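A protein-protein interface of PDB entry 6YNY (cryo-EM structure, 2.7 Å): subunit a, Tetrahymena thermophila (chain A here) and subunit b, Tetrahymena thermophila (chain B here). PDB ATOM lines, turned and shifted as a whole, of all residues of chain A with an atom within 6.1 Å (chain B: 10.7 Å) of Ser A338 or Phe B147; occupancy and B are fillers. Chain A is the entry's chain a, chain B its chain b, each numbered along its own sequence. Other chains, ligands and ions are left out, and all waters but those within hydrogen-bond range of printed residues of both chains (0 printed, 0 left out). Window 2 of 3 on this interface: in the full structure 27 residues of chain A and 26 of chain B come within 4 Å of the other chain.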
ATOM      1  N   THR A 333     -26.734 -23.106 -12.510  1.00  0.00           N
ATOM      2  CA  THR A 333     -27.481 -21.897 -12.199  1.00  0.00           C
ATOM      3  C   THR A 333     -26.905 -21.180 -10.987  1.00  0.00           C
ATOM      4  O   THR A 333     -26.983 -19.950 -10.899  1.00  0.00           O
ATOM      5  CB  THR A 333     -28.948 -22.243 -11.961  1.00  0.00           C
ATOM      6  OG1 THR A 333     -29.460 -22.964 -13.086  1.00  0.00           O
ATOM      7  CG2 THR A 333     -29.758 -20.992 -11.764  1.00  0.00           C
ATOM      8  N   PHE A 334     -26.331 -21.928 -10.049  1.00  0.00           N
ATOM      9  CA  PHE A 334     -25.712 -21.332  -8.875  1.00  0.00           C
ATOM     10  C   PHE A 334     -24.369 -20.695  -9.203  1.00  0.00           C
ATOM     11  O   PHE A 334     -23.993 -19.697  -8.581  1.00  0.00           O
ATOM     12  CB  PHE A 334     -25.553 -22.397  -7.792  1.00  0.00           C
ATOM     13  CG  PHE A 334     -24.943 -21.896  -6.525  1.00  0.00           C
ATOM     14  CD1 PHE A 334     -25.689 -21.168  -5.623  1.00  0.00           C
ATOM     15  CD2 PHE A 334     -23.625 -22.169  -6.227  1.00  0.00           C
ATOM     16  CE1 PHE A 334     -25.128 -20.714  -4.457  1.00  0.00           C
ATOM     17  CE2 PHE A 334     -23.063 -21.717  -5.059  1.00  0.00           C
ATOM     18  CZ  PHE A 334     -23.816 -20.992  -4.175  1.00  0.00           C
ATOM     19  N   ILE A 335     -23.640 -21.251 -10.171  1.00  0.00           N
ATOM     20  CA  ILE A 335     -22.350 -20.688 -10.548  1.00  0.00           C
ATOM     21  C   ILE A 335     -22.533 -19.399 -11.337  1.00  0.00           C
ATOM     22  O   ILE A 335     -21.771 -18.439 -11.170  1.00  0.00           O
ATOM     23  CB  ILE A 335     -21.535 -21.725 -11.342  1.00  0.00           C
ATOM     24  CG1 ILE A 335     -21.210 -22.940 -10.472  1.00  0.00           C
ATOM     25  CG2 ILE A 335     -20.273 -21.111 -11.886  1.00  0.00           C
ATOM     26  CD1 ILE A 335     -20.478 -22.625  -9.204  1.00  0.00           C
ATOM     27  N   SER A 336     -23.536 -19.353 -12.215  1.00  0.00           N
ATOM     28  CA  SER A 336     -23.764 -18.150 -13.006  1.00  0.00           C
ATOM     29  C   SER A 336     -24.060 -16.949 -12.121  1.00  0.00           C
ATOM     30  O   SER A 336     -23.669 -15.824 -12.450  1.00  0.00           O
ATOM     31  CB  SER A 336     -24.908 -18.378 -13.989  1.00  0.00           C
ATOM     32  OG  SER A 336     -26.098 -18.722 -13.310  1.00  0.00           O
ATOM     33  N   LEU A 337     -24.753 -17.166 -11.004  1.00  0.00           N
ATOM     34  CA  LEU A 337     -25.026 -16.077 -10.077  1.00  0.00           C
ATOM     35  C   LEU A 337     -23.757 -15.626  -9.367  1.00  0.00           C
ATOM     36  O   LEU A 337     -23.542 -14.425  -9.173  1.00  0.00           O
ATOM     37  CB  LEU A 337     -26.082 -16.513  -9.067  1.00  0.00           C
ATOM     38  CG  LEU A 337     -26.480 -15.490  -8.008  1.00  0.00           C
ATOM     39  CD1 LEU A 337     -27.028 -14.242  -8.654  1.00  0.00           C
ATOM     40  CD2 LEU A 337     -27.495 -16.085  -7.067  1.00  0.00           C
ATOM     41  N   SER A 338     -22.907 -16.574  -8.970  1.00  0.00           N
ATOM     42  CA  SER A 338     -21.647 -16.214  -8.333  1.00  0.00           C
ATOM     43  C   SER A 338     -20.746 -15.455  -9.292  1.00  0.00           C
ATOM     44  O   SER A 338     -20.020 -14.542  -8.885  1.00  0.00           O
ATOM     45  CB  SER A 338     -20.948 -17.472  -7.826  1.00  0.00           C
ATOM     46  OG  SER A 338     -21.783 -18.201  -6.952  1.00  0.00           O
ATOM     47  N   HIS A 339     -20.780 -15.817 -10.575  1.00  0.00           N
ATOM     48  CA  HIS A 339     -19.973 -15.116 -11.563  1.00  0.00           C
ATOM     49  C   HIS A 339     -20.461 -13.692 -11.775  1.00  0.00           C
ATOM     50  O   HIS A 339     -19.653 -12.793 -12.025  1.00  0.00           O
ATOM     51  CB  HIS A 339     -19.986 -15.892 -12.878  1.00  0.00           C
ATOM     52  CG  HIS A 339     -19.417 -15.136 -14.035  1.00  0.00           C
ATOM     53  ND1 HIS A 339     -18.063 -15.025 -14.260  1.00  0.00           N
ATOM     54  CD2 HIS A 339     -20.021 -14.457 -15.037  1.00  0.00           C
ATOM     55  CE1 HIS A 339     -17.856 -14.308 -15.349  1.00  0.00           C
ATOM     56  NE2 HIS A 339     -19.028 -13.950 -15.840  1.00  0.00           N
ATOM     57  N   TYR A 340     -21.769 -13.464 -11.672  1.00  0.00           N
ATOM     58  CA  TYR A 340     -22.298 -12.119 -11.853  1.00  0.00           C
ATOM     59  C   TYR A 340     -22.025 -11.247 -10.636  1.00  0.00           C
ATOM     60  O   TYR A 340     -21.744 -10.053 -10.774  1.00  0.00           O
ATOM     61  CB  TYR A 340     -23.797 -12.185 -12.140  1.00  0.00           C
ATOM     62  CG  TYR A 340     -24.405 -10.861 -12.519  1.00  0.00           C
ATOM     63  CD1 TYR A 340     -25.079 -10.092 -11.588  1.00  0.00           C
ATOM     64  CD2 TYR A 340     -24.298 -10.376 -13.810  1.00  0.00           C
ATOM     65  CE1 TYR A 340     -25.632  -8.883 -11.932  1.00  0.00           C
ATOM     66  CE2 TYR A 340     -24.846  -9.168 -14.162  1.00  0.00           C
ATOM     67  CZ  TYR A 340     -25.511  -8.425 -13.219  1.00  0.00           C
ATOM     68  OH  TYR A 340     -26.061  -7.219 -13.568  1.00  0.00           O
ATOM     69  N   VAL A 341     -22.097 -11.830  -9.442  1.00  0.00           N
ATOM     70  CA  VAL A 341     -21.860 -11.071  -8.221  1.00  0.00           C
ATOM     71  C   VAL A 341     -20.377 -10.801  -8.031  1.00  0.00           C
ATOM     72  O   VAL A 341     -19.979  -9.689  -7.666  1.00  0.00           O
ATOM     73  CB  VAL A 341     -22.458 -11.817  -7.018  1.00  0.00           C
ATOM     74  CG1 VAL A 341     -22.064 -11.145  -5.731  1.00  0.00           C
ATOM     75  CG2 VAL A 341     -23.955 -11.883  -7.143  1.00  0.00           C
ATOM     76  N   SER A 342     -19.534 -11.807  -8.265  1.00  0.00           N
ATOM     77  CA  SER A 342     -18.102 -11.621  -8.076  1.00  0.00           C
ATOM     78  C   SER A 342     -17.526 -10.646  -9.092  1.00  0.00           C
ATOM     79  O   SER A 342     -16.522  -9.983  -8.815  1.00  0.00           O
ATOM     80  CB  SER A 342     -17.388 -12.967  -8.158  1.00  0.00           C
ATOM     81  OG  SER A 342     -17.513 -13.544  -9.443  1.00  0.00           O
ATOM     82  N   ASP A 343     -18.147 -10.541 -10.264  1.00  0.00           N
ATOM     83  CA  ASP A 343     -17.717  -9.621 -11.304  1.00  0.00           C
ATOM     84  C   ASP A 343     -18.564  -8.360 -11.356  1.00  0.00           C
ATOM     85  O   ASP A 343     -18.478  -7.608 -12.330  1.00  0.00           O
ATOM     86  CB  ASP A 343     -17.747 -10.319 -12.663  1.00  0.00           C
ATOM     87  CG  ASP A 343     -16.746 -11.455 -12.758  1.00  0.00           C
ATOM     88  OD1 ASP A 343     -16.929 -12.474 -12.060  1.00  0.00           O
ATOM     89  OD2 ASP A 343     -15.777 -11.331 -13.535  1.00  0.00           O
ATOM     90  N   SER B 140     -10.336  -8.642   0.449  1.00  0.00           N
ATOM     91  CA  SER B 140     -10.570 -10.066   0.267  1.00  0.00           C
ATOM     92  C   SER B 140     -11.880 -10.523   0.890  1.00  0.00           C
ATOM     93  O   SER B 140     -12.273 -11.677   0.692  1.00  0.00           O
ATOM     94  CB  SER B 140      -9.401 -10.857   0.850  1.00  0.00           C
ATOM     95  OG  SER B 140      -8.189 -10.508   0.217  1.00  0.00           O
ATOM     96  N   THR B 141     -12.563  -9.650   1.627  1.00  0.00           N
ATOM     97  CA  THR B 141     -13.840  -9.959   2.248  1.00  0.00           C
ATOM     98  C   THR B 141     -15.023  -9.344   1.514  1.00  0.00           C
ATOM     99  O   THR B 141     -16.168  -9.678   1.831  1.00  0.00           O
ATOM    100  CB  THR B 141     -13.839  -9.475   3.704  1.00  0.00           C
ATOM    101  OG1 THR B 141     -12.695  -9.996   4.384  1.00  0.00           O
ATOM    102  CG2 THR B 141     -15.084  -9.922   4.424  1.00  0.00           C
ATOM    103  N   TYR B 142     -14.780  -8.473   0.536  1.00  0.00           N
ATOM    104  CA  TYR B 142     -15.875  -7.775  -0.125  1.00  0.00           C
ATOM    105  C   TYR B 142     -16.803  -8.743  -0.845  1.00  0.00           C
ATOM    106  O   TYR B 142     -18.023  -8.709  -0.655  1.00  0.00           O
ATOM    107  CB  TYR B 142     -15.318  -6.741  -1.101  1.00  0.00           C
ATOM    108  CG  TYR B 142     -16.383  -6.003  -1.867  1.00  0.00           C
ATOM    109  CD1 TYR B 142     -17.069  -4.950  -1.291  1.00  0.00           C
ATOM    110  CD2 TYR B 142     -16.702  -6.357  -3.167  1.00  0.00           C
ATOM    111  CE1 TYR B 142     -18.040  -4.273  -1.984  1.00  0.00           C
ATOM    112  CE2 TYR B 142     -17.672  -5.687  -3.866  1.00  0.00           C
ATOM    113  CZ  TYR B 142     -18.339  -4.645  -3.271  1.00  0.00           C
ATOM    114  OH  TYR B 142     -19.309  -3.972  -3.970  1.00  0.00           O
ATOM    115  N   ILE B 143     -16.242  -9.613  -1.681  1.00  0.00           N
ATOM    116  CA  ILE B 143     -17.074 -10.520  -2.470  1.00  0.00           C
ATOM    117  C   ILE B 143     -17.939 -11.408  -1.585  1.00  0.00           C
ATOM    118  O   ILE B 143     -19.163 -11.442  -1.793  1.00  0.00           O
ATOM    119  CB  ILE B 143     -16.194 -11.333  -3.437  1.00  0.00           C
ATOM    120  CG1 ILE B 143     -15.613 -10.418  -4.510  1.00  0.00           C
ATOM    121  CG2 ILE B 143     -17.000 -12.441  -4.066  1.00  0.00           C
ATOM    122  CD1 ILE B 143     -14.499 -11.030  -5.304  1.00  0.00           C
ATOM    123  N   PRO B 144     -17.398 -12.144  -0.614  1.00  0.00           N
ATOM    124  CA  PRO B 144     -18.267 -12.974   0.228  1.00  0.00           C
ATOM    125  C   PRO B 144     -19.293 -12.181   1.011  1.00  0.00           C
ATOM    126  O   PRO B 144     -20.352 -12.720   1.346  1.00  0.00           O
ATOM    127  CB  PRO B 144     -17.273 -13.695   1.149  1.00  0.00           C
ATOM    128  CG  PRO B 144     -16.036 -12.919   1.075  1.00  0.00           C
ATOM    129  CD  PRO B 144     -15.982 -12.326  -0.277  1.00  0.00           C
ATOM    130  N   TRP B 145     -19.013 -10.914   1.316  1.00  0.00           N
ATOM    131  CA  TRP B 145     -19.997 -10.095   2.010  1.00  0.00           C
ATOM    132  C   TRP B 145     -21.201  -9.819   1.122  1.00  0.00           C
ATOM    133  O   TRP B 145     -22.346  -9.899   1.576  1.00  0.00           O
ATOM    134  CB  TRP B 145     -19.359  -8.791   2.473  1.00  0.00           C
ATOM    135  CG  TRP B 145     -20.200  -8.029   3.435  1.00  0.00           C
ATOM    136  CD1 TRP B 145     -21.010  -6.975   3.156  1.00  0.00           C
ATOM    137  CD2 TRP B 145     -20.319  -8.265   4.839  1.00  0.00           C
ATOM    138  NE1 TRP B 145     -21.627  -6.539   4.297  1.00  0.00           N
ATOM    139  CE2 TRP B 145     -21.218  -7.316   5.346  1.00  0.00           C
ATOM    140  CE3 TRP B 145     -19.751  -9.188   5.716  1.00  0.00           C
ATOM    141  CZ2 TRP B 145     -21.563  -7.262   6.690  1.00  0.00           C
ATOM    142  CZ3 TRP B 145     -20.094  -9.133   7.045  1.00  0.00           C
ATOM    143  CH2 TRP B 145     -20.991  -8.178   7.521  1.00  0.00           C
ATOM    144  N   ILE B 146     -20.964  -9.499  -0.148  1.00  0.00           N
ATOM    145  CA  ILE B 146     -22.070  -9.240  -1.061  1.00  0.00           C
ATOM    146  C   ILE B 146     -22.793 -10.535  -1.394  1.00  0.00           C
ATOM    147  O   ILE B 146     -24.027 -10.588  -1.406  1.00  0.00           O
ATOM    148  CB  ILE B 146     -21.564  -8.548  -2.338  1.00  0.00           C
ATOM    149  CG1 ILE B 146     -20.693  -7.336  -2.016  1.00  0.00           C
ATOM    150  CG2 ILE B 146     -22.728  -8.123  -3.190  1.00  0.00           C
ATOM    151  CD1 ILE B 146     -21.423  -6.180  -1.424  1.00  0.00           C
ATOM    152  N   PHE B 147     -22.037 -11.600  -1.660  1.00  0.00           N
ATOM    153  CA  PHE B 147     -22.631 -12.839  -2.147  1.00  0.00           C
ATOM    154  C   PHE B 147     -23.593 -13.436  -1.129  1.00  0.00           C
ATOM    155  O   PHE B 147     -24.741 -13.753  -1.456  1.00  0.00           O
ATOM    156  CB  PHE B 147     -21.530 -13.840  -2.491  1.00  0.00           C
ATOM    157  CG  PHE B 147     -22.044 -15.171  -2.918  1.00  0.00           C
ATOM    158  CD1 PHE B 147     -22.541 -15.359  -4.187  1.00  0.00           C
ATOM    159  CD2 PHE B 147     -22.036 -16.238  -2.046  1.00  0.00           C
ATOM    160  CE1 PHE B 147     -23.016 -16.583  -4.576  1.00  0.00           C
ATOM    161  CE2 PHE B 147     -22.507 -17.458  -2.432  1.00  0.00           C
ATOM    162  CZ  PHE B 147     -22.999 -17.632  -3.697  1.00  0.00           C
ATOM    163  N   TRP B 148     -23.140 -13.609   0.110  1.00  0.00           N
ATOM    164  CA  TRP B 148     -23.959 -14.310   1.090  1.00  0.00           C
ATOM    165  C   TRP B 148     -25.133 -13.468   1.560  1.00  0.00           C
ATOM    166  O   TRP B 148     -26.169 -14.019   1.943  1.00  0.00           O
ATOM    167  CB  TRP B 148     -23.101 -14.738   2.273  1.00  0.00           C
ATOM    168  CG  TRP B 148     -22.176 -15.852   1.941  1.00  0.00           C
ATOM    169  CD1 TRP B 148     -20.822 -15.810   1.925  1.00  0.00           C
ATOM    170  CD2 TRP B 148     -22.542 -17.178   1.557  1.00  0.00           C
ATOM    171  NE1 TRP B 148     -20.314 -17.028   1.563  1.00  0.00           N
ATOM    172  CE2 TRP B 148     -21.352 -17.887   1.332  1.00  0.00           C
ATOM    173  CE3 TRP B 148     -23.759 -17.835   1.386  1.00  0.00           C
ATOM    174  CZ2 TRP B 148     -21.343 -19.219   0.946  1.00  0.00           C
ATOM    175  CZ3 TRP B 148     -23.747 -19.155   1.004  1.00  0.00           C
ATOM    176  CH2 TRP B 148     -22.549 -19.833   0.787  1.00  0.00           C
ATOM    177  N   PHE B 149     -25.005 -12.145   1.529  1.00  0.00           N
ATOM    178  CA  PHE B 149     -26.112 -11.298   1.951  1.00  0.00           C
ATOM    179  C   PHE B 149     -27.169 -11.172   0.862  1.00  0.00           C
ATOM    180  O   PHE B 149     -28.367 -11.174   1.160  1.00  0.00           O
ATOM    181  CB  PHE B 149     -25.591  -9.926   2.368  1.00  0.00           C
ATOM    182  CG  PHE B 149     -25.152  -9.859   3.797  1.00  0.00           C
ATOM    183  CD1 PHE B 149     -26.047  -9.522   4.790  1.00  0.00           C
ATOM    184  CD2 PHE B 149     -23.847 -10.134   4.151  1.00  0.00           C
ATOM    185  CE1 PHE B 149     -25.652  -9.461   6.098  1.00  0.00           C
ATOM    186  CE2 PHE B 149     -23.451 -10.073   5.460  1.00  0.00           C
ATOM    187  CZ  PHE B 149     -24.356  -9.737   6.435  1.00  0.00           C
ATOM    188  N   GLN B 150     -26.756 -11.072  -0.401  1.00  0.00           N
ATOM    189  CA  GLN B 150     -27.730 -10.994  -1.480  1.00  0.00           C
ATOM    190  C   GLN B 150     -28.410 -12.330  -1.730  1.00  0.00           C
ATOM    191  O   GLN B 150     -29.510 -12.355  -2.286  1.00  0.00           O
ATOM    192  CB  GLN B 150     -27.065 -10.496  -2.762  1.00  0.00           C
ATOM    193  CG  GLN B 150     -26.011 -11.418  -3.346  1.00  0.00           C
ATOM    194  CD  GLN B 150     -26.575 -12.469  -4.274  1.00  0.00           C
ATOM    195  OE1 GLN B 150     -27.544 -12.230  -4.988  1.00  0.00           O
ATOM    196  NE2 GLN B 150     -25.965 -13.645  -4.269  1.00  0.00           N
ATOM    197  N   LEU B 151     -27.788 -13.433  -1.327  1.00  0.00           N
ATOM    198  CA  LEU B 151     -28.354 -14.754  -1.554  1.00  0.00           C
ATOM    199  C   LEU B 151     -29.297 -15.173  -0.435  1.00  0.00           C
ATOM    200  O   LEU B 151     -30.313 -15.827  -0.693  1.00  0.00           O
ATOM    201  CB  LEU B 151     -27.233 -15.782  -1.694  1.00  0.00           C
ATOM    202  CG  LEU B 151     -27.649 -17.164  -2.183  1.00  0.00           C
ATOM    203  CD1 LEU B 151     -28.056 -17.110  -3.637  1.00  0.00           C
ATOM    204  CD2 LEU B 151     -26.524 -18.136  -1.985  1.00  0.00           C
ATOM    205  N   MET B 152     -28.978 -14.808   0.803  1.00  0.00           N
ATOM    206  CA  MET B 152     -29.738 -15.209   1.976  1.00  0.00           C
ATOM    207  C   MET B 152     -30.657 -14.112   2.495  1.00  0.00           C
ATOM    208  O   MET B 152     -31.242 -14.269   3.568  1.00  0.00           O
ATOM    209  CB  MET B 152     -28.784 -15.652   3.084  1.00  0.00           C
ATOM    210  CG  MET B 152     -28.067 -16.965   2.821  1.00  0.00           C
ATOM    211  SD  MET B 152     -29.148 -18.401   2.853  1.00  0.00           S
ATOM    212  CE  MET B 152     -29.557 -18.569   1.123  1.00  0.00           C
ATOM    213  N   TYR B 153     -30.807 -13.012   1.758  1.00  0.00           N
ATOM    214  CA  TYR B 153     -31.647 -11.917   2.231  1.00  0.00           C
ATOM    215  C   TYR B 153     -33.098 -12.353   2.370  1.00  0.00           C
ATOM    216  O   TYR B 153     -33.745 -12.082   3.388  1.00  0.00           O
ATOM    217  CB  TYR B 153     -31.541 -10.724   1.287  1.00  0.00           C
ATOM    218  CG  TYR B 153     -32.614  -9.692   1.519  1.00  0.00           C
ATOM    219  CD1 TYR B 153     -32.569  -8.858   2.621  1.00  0.00           C
ATOM    220  CD2 TYR B 153     -33.675  -9.557   0.642  1.00  0.00           C
ATOM    221  CE1 TYR B 153     -33.544  -7.922   2.842  1.00  0.00           C
ATOM    222  CE2 TYR B 153     -34.657  -8.622   0.857  1.00  0.00           C
ATOM    223  CZ  TYR B 153     -34.587  -7.807   1.958  1.00  0.00           C
ATOM    224  OH  TYR B 153     -35.566  -6.870   2.179  1.00  0.00           O
ATOM    225  N   PHE B 154     -33.631 -13.028   1.352  1.00  0.00           N
ATOM    226  CA  PHE B 154     -35.043 -13.389   1.364  1.00  0.00           C
ATOM    227  C   PHE B 154     -35.364 -14.342   2.505  1.00  0.00           C
ATOM    228  O   PHE B 154     -36.338 -14.145   3.239  1.00  0.00           O
ATOM    229  CB  PHE B 154     -35.434 -14.009   0.026  1.00  0.00           C
ATOM    230  CG  PHE B 154     -36.827 -14.548   0.005  1.00  0.00           C
ATOM    231  CD1 PHE B 154     -37.898 -13.719  -0.246  1.00  0.00           C
ATOM    232  CD2 PHE B 154     -37.068 -15.884   0.251  1.00  0.00           C
ATOM    233  CE1 PHE B 154     -39.176 -14.212  -0.256  1.00  0.00           C
ATOM    234  CE2 PHE B 154     -38.346 -16.378   0.244  1.00  0.00           C
ATOM    235  CZ  PHE B 154     -39.399 -15.542  -0.012  1.00  0.00           C
ATOM    236  N   TYR B 155     -34.554 -15.386   2.671  1.00  0.00           N
ATOM    237  CA  TYR B 155     -34.827 -16.401   3.678  1.00  0.00           C
ATOM    238  C   TYR B 155     -34.654 -15.890   5.098  1.00  0.00           C
ATOM    239  O   TYR B 155     -35.084 -16.569   6.036  1.00  0.00           O
ATOM    240  CB  TYR B 155     -33.925 -17.612   3.453  1.00  0.00           C
ATOM    241  CG  TYR B 155     -34.064 -18.223   2.083  1.00  0.00           C
ATOM    242  CD1 TYR B 155     -35.069 -19.132   1.810  1.00  0.00           C
ATOM    243  CD2 TYR B 155     -33.189 -17.890   1.064  1.00  0.00           C
ATOM    244  CE1 TYR B 155     -35.200 -19.691   0.561  1.00  0.00           C
ATOM    245  CE2 TYR B 155     -33.312 -18.445  -0.188  1.00  0.00           C
ATOM    246  CZ  TYR B 155     -34.318 -19.345  -0.435  1.00  0.00           C
ATOM    247  OH  TYR B 155     -34.443 -19.899  -1.685  1.00  0.00           O
ATOM    248  N   VAL B 156     -34.048 -14.726   5.283  1.00  0.00           N
ATOM    249  CA  VAL B 156     -33.805 -14.157   6.600  1.00  0.00           C
ATOM    250  C   VAL B 156     -34.735 -12.982   6.876  1.00  0.00           C
ATOM    251  O   VAL B 156     -35.377 -12.920   7.924  1.00  0.00           O
ATOM    252  CB  VAL B 156     -32.327 -13.738   6.750  1.00  0.00           C
ATOM    253  CG1 VAL B 156     -32.100 -13.073   8.081  1.00  0.00           C
ATOM    254  CG2 VAL B 156     -31.422 -14.938   6.597  1.00  0.00           C
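The backbone carbonyl oxygen of Ser A338 sits at hydrogen-bond distance from the side-chain hydroxyl of Ser A342, 2.8 Å away.
The backbone carbonyl oxygen (O) of Phe B147 is in hydrogen-bond range of the side-chain amide nitrogen (NE2) of Gln B150.
The side-chain hydroxyl (OG) of Ser A338 lies within hydrogen-bond range of the backbone carbonyl oxygen (O) of Phe A334 (3.1 Å).
Among the printed residues, pairs that only touch across the chains: Phe A334 with Phe B147, Phe A334 with Leu B151, Leu A337 with Leu B151, Ser A338 with Phe B147 and Val A341 with Gln B150.
Of the 11 printed residues of chain A, 4 touch a printed residue of chain B.
Printed residues of chain A that touch a printed residue of chain B: Phe A334, Leu A337, Ser A338 and Val A341.
Hydrophobic or aromatic side chains of chain A within 4 Å of the printed part of chain B: Phe A334, Leu A337 and Val A341.
Of the 17 printed residues of chain B, 3 touch a printed residue of chain A.
Printed residues of chain B that touch a printed residue of chain A: Phe B147, Gln B150 and Leu B151.
Hydrophobic or aromatic side chains of chain B within 4 Å of the printed part of chain A: Phe B147 and Leu B151.
Of chain B, only Phe B147 comes within 4 Å of Ser A338.
Of the printed residues of chain A, Phe B147 touches Phe A334 and Ser A338.
Phe A334 touches just these residues of chain B: Phe B147 (3.5 Å) and Leu B151 (3.8 Å).
No residue of chain B comes within 4 Å of Ile A335.
No residue of chain B comes within 4 Å of Ser A336.
No residue of chain B comes within 4 Å of Ser A342.
Printed residues of chain B within 4 Å of Leu A337: Leu B151 (3.6 Å).
Of the printed residues of chain A, Gln B150 touches Val A341 (3.9 Å).
Of the printed residues of chain B, Val A341 touches Gln B150.
Phe B154 touches none of the printed residues of chain A.
The nearest printed residue of chain A that does not touch Phe B147 is Val A341 (4.005 Å).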
